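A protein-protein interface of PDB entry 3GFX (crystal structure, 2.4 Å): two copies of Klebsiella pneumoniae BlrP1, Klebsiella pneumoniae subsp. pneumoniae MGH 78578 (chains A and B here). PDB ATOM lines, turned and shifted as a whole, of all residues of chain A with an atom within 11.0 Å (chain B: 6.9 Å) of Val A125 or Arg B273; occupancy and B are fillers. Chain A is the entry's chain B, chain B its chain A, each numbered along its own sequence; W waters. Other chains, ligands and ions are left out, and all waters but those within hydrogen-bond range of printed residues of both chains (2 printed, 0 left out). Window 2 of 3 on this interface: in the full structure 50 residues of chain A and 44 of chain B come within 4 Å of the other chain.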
ATOM      1  N   ALA A  91     -25.437  10.045  -6.474  1.00  0.00           N
ATOM      2  CA  ALA A  91     -25.093   9.211  -7.627  1.00  0.00           C
ATOM      3  C   ALA A  91     -24.421   7.896  -7.235  1.00  0.00           C
ATOM      4  O   ALA A  91     -24.419   6.939  -8.014  1.00  0.00           O
ATOM      5  CB  ALA A  91     -24.221   9.980  -8.595  1.00  0.00           C
ATOM      6  N   TYR A  92     -23.849   7.857  -6.035  1.00  0.00           N
ATOM      7  CA  TYR A  92     -23.159   6.668  -5.538  1.00  0.00           C
ATOM      8  C   TYR A  92     -23.193   6.603  -4.013  1.00  0.00           C
ATOM      9  O   TYR A  92     -23.305   7.629  -3.340  1.00  0.00           O
ATOM     10  CB  TYR A  92     -21.709   6.613  -6.054  1.00  0.00           C
ATOM     11  CG  TYR A  92     -20.806   7.714  -5.535  1.00  0.00           C
ATOM     12  CD1 TYR A  92     -20.734   8.947  -6.177  1.00  0.00           C
ATOM     13  CD2 TYR A  92     -20.010   7.515  -4.408  1.00  0.00           C
ATOM     14  CE1 TYR A  92     -19.906   9.954  -5.705  1.00  0.00           C
ATOM     15  CE2 TYR A  92     -19.178   8.515  -3.928  1.00  0.00           C
ATOM     16  CZ  TYR A  92     -19.131   9.733  -4.581  1.00  0.00           C
ATOM     17  OH  TYR A  92     -18.309  10.731  -4.111  1.00  0.00           O
ATOM     18  N   ARG A  93     -23.101   5.390  -3.475  1.00  0.00           N
ATOM     19  CA  ARG A  93     -23.052   5.194  -2.031  1.00  0.00           C
ATOM     20  C   ARG A  93     -21.649   5.460  -1.504  1.00  0.00           C
ATOM     21  O   ARG A  93     -20.661   4.986  -2.068  1.00  0.00           O
ATOM     22  CB  ARG A  93     -23.496   3.777  -1.655  1.00  0.00           C
ATOM     23  CG  ARG A  93     -24.982   3.525  -1.837  1.00  0.00           C
ATOM     24  CD  ARG A  93     -25.340   2.097  -1.481  1.00  0.00           C
ATOM     25  NE  ARG A  93     -26.693   1.755  -1.911  1.00  0.00           N
ATOM     26  CZ  ARG A  93     -27.779   1.881  -1.155  1.00  0.00           C
ATOM     27  NH1 ARG A  93     -27.686   2.342   0.086  1.00  0.00           N
ATOM     28  NH2 ARG A  93     -28.965   1.541  -1.642  1.00  0.00           N
ATOM     29  N   ARG A  94     -21.569   6.227  -0.422  1.00  0.00           N
ATOM     30  CA  ARG A  94     -20.291   6.527   0.205  1.00  0.00           C
ATOM     31  C   ARG A  94     -19.886   5.423   1.173  1.00  0.00           C
ATOM     32  O   ARG A  94     -18.700   5.173   1.376  1.00  0.00           O
ATOM     33  CB  ARG A  94     -20.337   7.878   0.926  1.00  0.00           C
ATOM     34  CG  ARG A  94     -19.978   9.087   0.064  1.00  0.00           C
ATOM     35  CD  ARG A  94     -21.063   9.448  -0.939  1.00  0.00           C
ATOM     36  NE  ARG A  94     -20.837  10.763  -1.532  1.00  0.00           N
ATOM     37  CZ  ARG A  94     -21.523  11.252  -2.560  1.00  0.00           C
ATOM     38  NH1 ARG A  94     -22.488  10.536  -3.125  1.00  0.00           N
ATOM     39  NH2 ARG A  94     -21.243  12.462  -3.024  1.00  0.00           N
ATOM     40  N   SER A 121     -14.904   3.764   3.533  1.00  0.00           N
ATOM     41  CA  SER A 121     -15.752   4.689   2.787  1.00  0.00           C
ATOM     42  C   SER A 121     -15.143   5.125   1.461  1.00  0.00           C
ATOM     43  O   SER A 121     -13.932   5.282   1.346  1.00  0.00           O
ATOM     44  CB  SER A 121     -16.095   5.915   3.633  1.00  0.00           C
ATOM     45  OG  SER A 121     -14.930   6.660   3.928  1.00  0.00           O
ATOM     46  N   THR A 122     -16.003   5.311   0.461  1.00  0.00           N
ATOM     47  CA  THR A 122     -15.582   5.773  -0.860  1.00  0.00           C
ATOM     48  C   THR A 122     -16.096   7.185  -1.110  1.00  0.00           C
ATOM     49  O   THR A 122     -17.291   7.444  -0.975  1.00  0.00           O
ATOM     50  CB  THR A 122     -16.101   4.853  -1.987  1.00  0.00           C
ATOM     51  OG1 THR A 122     -17.511   4.646  -1.831  1.00  0.00           O
ATOM     52  CG2 THR A 122     -15.390   3.511  -1.960  1.00  0.00           C
ATOM     53  N   PHE A 123     -15.196   8.093  -1.477  1.00  0.00           N
ATOM     54  CA  PHE A 123     -15.574   9.485  -1.738  1.00  0.00           C
ATOM     55  C   PHE A 123     -15.228   9.972  -3.151  1.00  0.00           C
ATOM     56  O   PHE A 123     -15.161  11.177  -3.394  1.00  0.00           O
ATOM     57  CB  PHE A 123     -14.967  10.425  -0.688  1.00  0.00           C
ATOM     58  CG  PHE A 123     -15.629  10.344   0.658  1.00  0.00           C
ATOM     59  CD1 PHE A 123     -16.892  10.887   0.860  1.00  0.00           C
ATOM     60  CD2 PHE A 123     -14.988   9.733   1.729  1.00  0.00           C
ATOM     61  CE1 PHE A 123     -17.511  10.817   2.106  1.00  0.00           C
ATOM     62  CE2 PHE A 123     -15.599   9.659   2.977  1.00  0.00           C
ATOM     63  CZ  PHE A 123     -16.863  10.201   3.165  1.00  0.00           C
ATOM     64  N   GLY A 124     -15.015   9.039  -4.075  1.00  0.00           N
ATOM     65  CA  GLY A 124     -14.772   9.387  -5.476  1.00  0.00           C
ATOM     66  C   GLY A 124     -13.308   9.503  -5.856  1.00  0.00           C
ATOM     67  O   GLY A 124     -12.423   9.139  -5.078  1.00  0.00           O
ATOM     68  N   VAL A 125     -13.054  10.015  -7.059  1.00  0.00           N
ATOM     69  CA  VAL A 125     -11.690  10.116  -7.588  1.00  0.00           C
ATOM     70  C   VAL A 125     -10.892  11.281  -7.002  1.00  0.00           C
ATOM     71  O   VAL A 125      -9.659  11.248  -6.990  1.00  0.00           O
ATOM     72  CB  VAL A 125     -11.656  10.182  -9.141  1.00  0.00           C
ATOM     73  CG1 VAL A 125     -12.012   8.830  -9.743  1.00  0.00           C
ATOM     74  CG2 VAL A 125     -12.571  11.281  -9.673  1.00  0.00           C
ATOM     75  N   THR A 126     -11.592  12.305  -6.520  1.00  0.00           N
ATOM     76  CA  THR A 126     -10.934  13.450  -5.893  1.00  0.00           C
ATOM     77  C   THR A 126     -10.816  13.247  -4.383  1.00  0.00           C
ATOM     78  O   THR A 126     -11.341  12.272  -3.834  1.00  0.00           O
ATOM     79  CB  THR A 126     -11.657  14.787  -6.200  1.00  0.00           C
ATOM     80  OG1 THR A 126     -12.940  14.810  -5.561  1.00  0.00           O
ATOM     81  CG2 THR A 126     -11.829  14.980  -7.707  1.00  0.00           C
ATOM     82  N   GLU A 127     -10.117  14.173  -3.727  1.00  0.00           N
ATOM     83  CA  GLU A 127      -9.894  14.147  -2.281  1.00  0.00           C
ATOM     84  C   GLU A 127     -11.230  14.173  -1.525  1.00  0.00           C
ATOM     85  O   GLU A 127     -12.156  14.862  -1.948  1.00  0.00           O
ATOM     86  CB  GLU A 127      -9.038  15.355  -1.882  1.00  0.00           C
ATOM     87  CG  GLU A 127      -7.866  15.033  -0.965  1.00  0.00           C
ATOM     88  CD  GLU A 127      -6.727  14.333  -1.685  1.00  0.00           C
ATOM     89  OE1 GLU A 127      -6.138  14.943  -2.604  1.00  0.00           O
ATOM     90  OE2 GLU A 127      -6.414  13.178  -1.324  1.00  0.00           O
ATOM     91  N   PRO A 128     -11.338  13.409  -0.415  1.00  0.00           N
ATOM     92  CA  PRO A 128     -12.570  13.334   0.385  1.00  0.00           C
ATOM     93  C   PRO A 128     -13.093  14.683   0.885  1.00  0.00           C
ATOM     94  O   PRO A 128     -14.296  14.828   1.105  1.00  0.00           O
ATOM     95  CB  PRO A 128     -12.162  12.461   1.576  1.00  0.00           C
ATOM     96  CG  PRO A 128     -11.048  11.637   1.061  1.00  0.00           C
ATOM     97  CD  PRO A 128     -10.289  12.535   0.139  1.00  0.00           C
ATOM     98  N   VAL A 129     -12.196  15.655   1.047  1.00  0.00           N
ATOM     99  CA  VAL A 129     -12.558  17.010   1.474  1.00  0.00           C
ATOM    100  C   VAL A 129     -13.413  17.750   0.426  1.00  0.00           C
ATOM    101  O   VAL A 129     -14.006  18.790   0.719  1.00  0.00           O
ATOM    102  CB  VAL A 129     -11.290  17.831   1.863  1.00  0.00           C
ATOM    103  CG1 VAL A 129     -10.570  18.366   0.626  1.00  0.00           C
ATOM    104  CG2 VAL A 129     -11.635  18.958   2.835  1.00  0.00           C
ATOM    105  N   ASN A 130     -13.485  17.197  -0.785  1.00  0.00           N
ATOM    106  CA  ASN A 130     -14.331  17.742  -1.846  1.00  0.00           C
ATOM    107  C   ASN A 130     -15.775  17.226  -1.794  1.00  0.00           C
ATOM    108  O   ASN A 130     -16.602  17.591  -2.631  1.00  0.00           O
ATOM    109  CB  ASN A 130     -13.715  17.463  -3.223  1.00  0.00           C
ATOM    110  CG  ASN A 130     -12.422  18.228  -3.451  1.00  0.00           C
ATOM    111  OD1 ASN A 130     -12.426  19.450  -3.584  1.00  0.00           O
ATOM    112  ND2 ASN A 130     -11.309  17.505  -3.506  1.00  0.00           N
ATOM    113  N   ASP A 131     -16.069  16.385  -0.803  1.00  0.00           N
ATOM    114  CA  ASP A 131     -17.408  15.833  -0.609  1.00  0.00           C
ATOM    115  C   ASP A 131     -18.090  16.528   0.568  1.00  0.00           C
ATOM    116  O   ASP A 131     -17.521  16.616   1.659  1.00  0.00           O
ATOM    117  CB  ASP A 131     -17.324  14.324  -0.360  1.00  0.00           C
ATOM    118  CG  ASP A 131     -18.608  13.590  -0.719  1.00  0.00           C
ATOM    119  OD1 ASP A 131     -19.664  13.868  -0.112  1.00  0.00           O
ATOM    120  OD2 ASP A 131     -18.554  12.711  -1.606  1.00  0.00           O
ATOM    121  N   LEU B 239      -5.299  15.654 -15.511  1.00  0.00           N
ATOM    122  CA  LEU B 239      -6.252  16.043 -14.471  1.00  0.00           C
ATOM    123  C   LEU B 239      -5.936  15.382 -13.131  1.00  0.00           C
ATOM    124  O   LEU B 239      -5.603  16.060 -12.161  1.00  0.00           O
ATOM    125  CB  LEU B 239      -7.691  15.730 -14.899  1.00  0.00           C
ATOM    126  CG  LEU B 239      -8.798  16.487 -14.160  1.00  0.00           C
ATOM    127  CD1 LEU B 239      -8.510  17.983 -14.122  1.00  0.00           C
ATOM    128  CD2 LEU B 239     -10.151  16.224 -14.793  1.00  0.00           C
ATOM    129  N   GLY B 240      -6.044  14.057 -13.090  1.00  0.00           N
ATOM    130  CA  GLY B 240      -5.765  13.300 -11.880  1.00  0.00           C
ATOM    131  C   GLY B 240      -6.876  13.424 -10.858  1.00  0.00           C
ATOM    132  O   GLY B 240      -8.043  13.174 -11.162  1.00  0.00           O
ATOM    133  N   LYS B 241      -6.510  13.817  -9.642  1.00  0.00           N
ATOM    134  CA  LYS B 241      -7.477  13.956  -8.553  1.00  0.00           C
ATOM    135  C   LYS B 241      -7.979  15.395  -8.414  1.00  0.00           C
ATOM    136  O   LYS B 241      -8.484  15.787  -7.360  1.00  0.00           O
ATOM    137  CB  LYS B 241      -6.869  13.474  -7.230  1.00  0.00           C
ATOM    138  CG  LYS B 241      -6.346  12.041  -7.261  1.00  0.00           C
ATOM    139  CD  LYS B 241      -5.667  11.672  -5.952  1.00  0.00           C
ATOM    140  CE  LYS B 241      -4.851  10.388  -6.083  1.00  0.00           C
ATOM    141  NZ  LYS B 241      -5.696   9.166  -6.228  1.00  0.00           N
ATOM    142  N   HIS B 242      -7.845  16.174  -9.484  1.00  0.00           N
ATOM    143  CA  HIS B 242      -8.255  17.575  -9.479  1.00  0.00           C
ATOM    144  C   HIS B 242      -9.631  17.761 -10.108  1.00  0.00           C
ATOM    145  O   HIS B 242      -9.995  17.050 -11.042  1.00  0.00           O
ATOM    146  CB  HIS B 242      -7.231  18.434 -10.223  1.00  0.00           C
ATOM    147  CG  HIS B 242      -5.854  18.369  -9.644  1.00  0.00           C
ATOM    148  ND1 HIS B 242      -4.857  17.581 -10.176  1.00  0.00           N
ATOM    149  CD2 HIS B 242      -5.307  18.996  -8.575  1.00  0.00           C
ATOM    150  CE1 HIS B 242      -3.755  17.726  -9.463  1.00  0.00           C
ATOM    151  NE2 HIS B 242      -4.001  18.579  -8.485  1.00  0.00           N
ATOM    152  N   MET B 264     -22.883  14.951 -19.498  1.00  0.00           N
ATOM    153  CA  MET B 264     -22.477  13.685 -18.897  1.00  0.00           C
ATOM    154  C   MET B 264     -21.773  12.771 -19.902  1.00  0.00           C
ATOM    155  O   MET B 264     -20.696  12.247 -19.617  1.00  0.00           O
ATOM    156  CB  MET B 264     -23.702  12.987 -18.290  1.00  0.00           C
ATOM    157  CG  MET B 264     -23.406  11.760 -17.432  1.00  0.00           C
ATOM    158  SD  MET B 264     -22.127  11.999 -16.183  1.00  0.00           S
ATOM    159  CE  MET B 264     -22.737  13.398 -15.265  1.00  0.00           C
ATOM    160  N   LEU B 267     -18.287  14.342 -20.973  1.00  0.00           N
ATOM    161  CA  LEU B 267     -17.212  14.266 -19.983  1.00  0.00           C
ATOM    162  C   LEU B 267     -16.712  12.834 -19.777  1.00  0.00           C
ATOM    163  O   LEU B 267     -15.525  12.621 -19.536  1.00  0.00           O
ATOM    164  CB  LEU B 267     -17.616  14.928 -18.653  1.00  0.00           C
ATOM    165  CG  LEU B 267     -18.672  14.327 -17.716  1.00  0.00           C
ATOM    166  CD1 LEU B 267     -18.062  13.346 -16.723  1.00  0.00           C
ATOM    167  CD2 LEU B 267     -19.371  15.437 -16.968  1.00  0.00           C
ATOM    168  N   LEU B 268     -17.621  11.863 -19.875  1.00  0.00           N
ATOM    169  CA  LEU B 268     -17.270  10.451 -19.719  1.00  0.00           C
ATOM    170  C   LEU B 268     -16.452   9.946 -20.902  1.00  0.00           C
ATOM    171  O   LEU B 268     -15.594   9.077 -20.745  1.00  0.00           O
ATOM    172  CB  LEU B 268     -18.524   9.588 -19.542  1.00  0.00           C
ATOM    173  CG  LEU B 268     -19.251   9.623 -18.192  1.00  0.00           C
ATOM    174  CD1 LEU B 268     -20.590   8.906 -18.298  1.00  0.00           C
ATOM    175  CD2 LEU B 268     -18.406   9.023 -17.072  1.00  0.00           C
ATOM    176  N   GLY B 271     -12.838  10.741 -20.509  1.00  0.00           N
ATOM    177  CA  GLY B 271     -12.149   9.983 -19.467  1.00  0.00           C
ATOM    178  C   GLY B 271     -12.346  10.548 -18.071  1.00  0.00           C
ATOM    179  O   GLY B 271     -11.703  10.102 -17.118  1.00  0.00           O
ATOM    180  N   LEU B 272     -13.246  11.514 -17.944  1.00  0.00           N
ATOM    181  CA  LEU B 272     -13.482  12.193 -16.672  1.00  0.00           C
ATOM    182  C   LEU B 272     -14.627  11.559 -15.887  1.00  0.00           C
ATOM    183  O   LEU B 272     -15.398  10.761 -16.424  1.00  0.00           O
ATOM    184  CB  LEU B 272     -13.758  13.686 -16.900  1.00  0.00           C
ATOM    185  CG  LEU B 272     -12.835  14.454 -17.853  1.00  0.00           C
ATOM    186  CD1 LEU B 272     -13.322  15.885 -18.051  1.00  0.00           C
ATOM    187  CD2 LEU B 272     -11.394  14.437 -17.361  1.00  0.00           C
ATOM    188  N   ARG B 273     -14.733  11.915 -14.619  1.00  0.00           N
ATOM    189  CA  ARG B 273     -15.792  11.413 -13.752  1.00  0.00           C
ATOM    190  C   ARG B 273     -16.796  12.524 -13.437  1.00  0.00           C
ATOM    191  O   ARG B 273     -16.427  13.700 -13.414  1.00  0.00           O
ATOM    192  CB  ARG B 273     -15.200  10.834 -12.461  1.00  0.00           C
ATOM    193  CG  ARG B 273     -14.250   9.654 -12.671  1.00  0.00           C
ATOM    194  CD  ARG B 273     -14.852   8.565 -13.560  1.00  0.00           C
ATOM    195  NE  ARG B 273     -16.053   7.966 -12.982  1.00  0.00           N
ATOM    196  CZ  ARG B 273     -16.842   7.101 -13.617  1.00  0.00           C
ATOM    197  NH1 ARG B 273     -16.567   6.725 -14.861  1.00  0.00           N
ATOM    198  NH2 ARG B 273     -17.912   6.612 -13.005  1.00  0.00           N
ATOM    199  N   PRO B 274     -18.077  12.159 -13.224  1.00  0.00           N
ATOM    200  CA  PRO B 274     -19.120  13.126 -12.856  1.00  0.00           C
ATOM    201  C   PRO B 274     -18.756  13.973 -11.635  1.00  0.00           C
ATOM    202  O   PRO B 274     -18.880  15.200 -11.680  1.00  0.00           O
ATOM    203  CB  PRO B 274     -20.325  12.238 -12.540  1.00  0.00           C
ATOM    204  CG  PRO B 274     -20.096  10.998 -13.320  1.00  0.00           C
ATOM    205  CD  PRO B 274     -18.618  10.792 -13.348  1.00  0.00           C
ATOM    206  N   ASP B 275     -18.284  13.322 -10.572  1.00  0.00           N
ATOM    207  CA  ASP B 275     -17.912  13.998  -9.322  1.00  0.00           C
ATOM    208  C   ASP B 275     -16.701  14.927  -9.470  1.00  0.00           C
ATOM    209  O   ASP B 275     -16.409  15.732  -8.587  1.00  0.00           O
ATOM    210  CB  ASP B 275     -17.663  12.973  -8.206  1.00  0.00           C
ATOM    211  CG  ASP B 275     -16.734  11.845  -8.635  1.00  0.00           C
ATOM    212  OD1 ASP B 275     -17.167  10.970  -9.417  1.00  0.00           O
ATOM    213  OD2 ASP B 275     -15.576  11.824  -8.174  1.00  0.00           O
ATOM    214  N   GLN B 276     -16.020  14.807 -10.603  1.00  0.00           N
ATOM    215  CA  GLN B 276     -14.826  15.580 -10.906  1.00  0.00           C
ATOM    216  C   GLN B 276     -15.177  16.903 -11.588  1.00  0.00           C
ATOM    217  O   GLN B 276     -14.382  17.842 -11.586  1.00  0.00           O
ATOM    218  CB  GLN B 276     -13.927  14.746 -11.817  1.00  0.00           C
ATOM    219  CG  GLN B 276     -12.461  15.074 -11.767  1.00  0.00           C
ATOM    220  CD  GLN B 276     -11.617  14.013 -12.437  1.00  0.00           C
ATOM    221  OE1 GLN B 276     -12.061  13.343 -13.371  1.00  0.00           O
ATOM    222  NE2 GLN B 276     -10.391  13.852 -11.963  1.00  0.00           N
ATOM    223  N   VAL B 277     -16.371  16.972 -12.172  1.00  0.00           N
ATOM    224  CA  VAL B 277     -16.815  18.165 -12.893  1.00  0.00           C
ATOM    225  C   VAL B 277     -17.768  19.008 -12.041  1.00  0.00           C
ATOM    226  O   VAL B 277     -18.737  18.496 -11.474  1.00  0.00           O
ATOM    227  CB  VAL B 277     -17.462  17.798 -14.253  1.00  0.00           C
ATOM    228  CG1 VAL B 277     -17.945  19.044 -14.992  1.00  0.00           C
ATOM    229  CG2 VAL B 277     -16.473  17.021 -15.115  1.00  0.00           C
ATOM    230  N   LEU B 278     -17.474  20.301 -11.955  1.00  0.00           N
ATOM    231  CA  LEU B 278     -18.286  21.234 -11.189  1.00  0.00           C
ATOM    232  C   LEU B 278     -18.830  22.353 -12.082  1.00  0.00           C
ATOM    233  O   LEU B 278     -18.089  22.943 -12.870  1.00  0.00           O
ATOM    234  CB  LEU B 278     -17.470  21.788 -10.014  1.00  0.00           C
ATOM    235  CG  LEU B 278     -17.994  22.962  -9.186  1.00  0.00           C
ATOM    236  CD1 LEU B 278     -17.747  22.729  -7.705  1.00  0.00           C
ATOM    237  CD2 LEU B 278     -17.338  24.252  -9.651  1.00  0.00           C
ATOM    238  N   GLY B 304     -24.371  13.211 -10.627  1.00  0.00           N
ATOM    239  CA  GLY B 304     -23.182  13.196  -9.779  1.00  0.00           C
ATOM    240  C   GLY B 304     -22.282  14.410  -9.889  1.00  0.00           C
ATOM    241  O   GLY B 304     -21.294  14.521  -9.161  1.00  0.00           O
ATOM    242  N   MET B 305     -22.620  15.318 -10.797  1.00  0.00           N
ATOM    243  CA  MET B 305     -21.849  16.544 -10.980  1.00  0.00           C
ATOM    244  C   MET B 305     -22.071  17.518  -9.829  1.00  0.00           C
ATOM    245  O   MET B 305     -23.099  17.473  -9.150  1.00  0.00           O
ATOM    246  CB  MET B 305     -22.178  17.202 -12.322  1.00  0.00           C
ATOM    247  CG  MET B 305     -21.660  16.424 -13.522  1.00  0.00           C
ATOM    248  SD  MET B 305     -21.912  17.249 -15.108  1.00  0.00           S
ATOM    249  CE  MET B 305     -23.676  17.059 -15.336  1.00  0.00           C
HETATM  250  O   HOH W   1     -14.414  12.728  -6.119  1.00  0.00           O
HETATM  251  O   HOH W   2      -9.140  18.352  -5.258  1.00  0.00           O
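OD2 of Asp B275 sits at hydrogen-bond distance from N of Val A125 (3.3 Å).
The backbone NH of Arg B273 sits at hydrogen-bond distance from the side-chain amide oxygen of Gln B276.
Ala A91 touches Gly B304 (CB to CA, 3.6 Å).
Asp B275 touches Gly A124.
Val A125 touches Lys B241.
CG1 of Val A125 touches CG of Arg B273, at 3.8 Å.
Lys B241 touches Thr A126 (O to CG2, 3.5 Å).
Of the printed residues of chain B, Val A125 touches Lys B241 (3.4 Å), Arg B273 (3.8 Å) and Asp B275 (3.3 Å).
Of chain A, only Val A125 (3.8 Å) comes within 4 Å of Arg B273.
Lys B241 touches just these residues of chain A: Val A125 (3.4 Å) and Thr A126 (3.5 Å).
No residue of chain A comes within 4 Å of Leu B268.
No residue of chain A comes within 4 Å of Gly B271.
No residue of chain A comes within 4 Å of Pro B274.
Of chain A, only Gly A124 and Val A125 come within 4 Å of Asp B275.
No residue of chain A comes within 4 Å of Val B277.
Printed residues of chain A within 4 Å of Gly B304: Ala A91 (3.6 Å).
Printed residues of chain B within 4 Å of Thr A126: Lys B241.
Printed residues of chain B within 4 Å of Ala A91: Gly B304 (3.6 Å).
Of the printed residues of chain B, Gly A124 touches Asp B275.
The nearest residue of chain A that does not touch Arg B273 is Gly A124 (6.9 Å).
The nearest printed residue of chain B that does not touch Ala A91 is Pro B274 (6.0 Å).
Of the 17 printed residues of chain B, 4 touch a printed residue of chain A.
Along chain B the printed residues that touch a printed residue of chain A span positions 241 to 304.
No position is printed for both chains.
Water W1 lies within hydrogen-bond range of the side-chain carboxylate of Asp B275, the side-chain hydroxyl of Thr A126, the backbone NH of Val A125 and the backbone carbonyl oxygen of Phe A123.
Water W2 lies within hydrogen-bond range of ND2 of Asn A130 (2.9 Å) and O of Lys B241 (3.4 Å).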
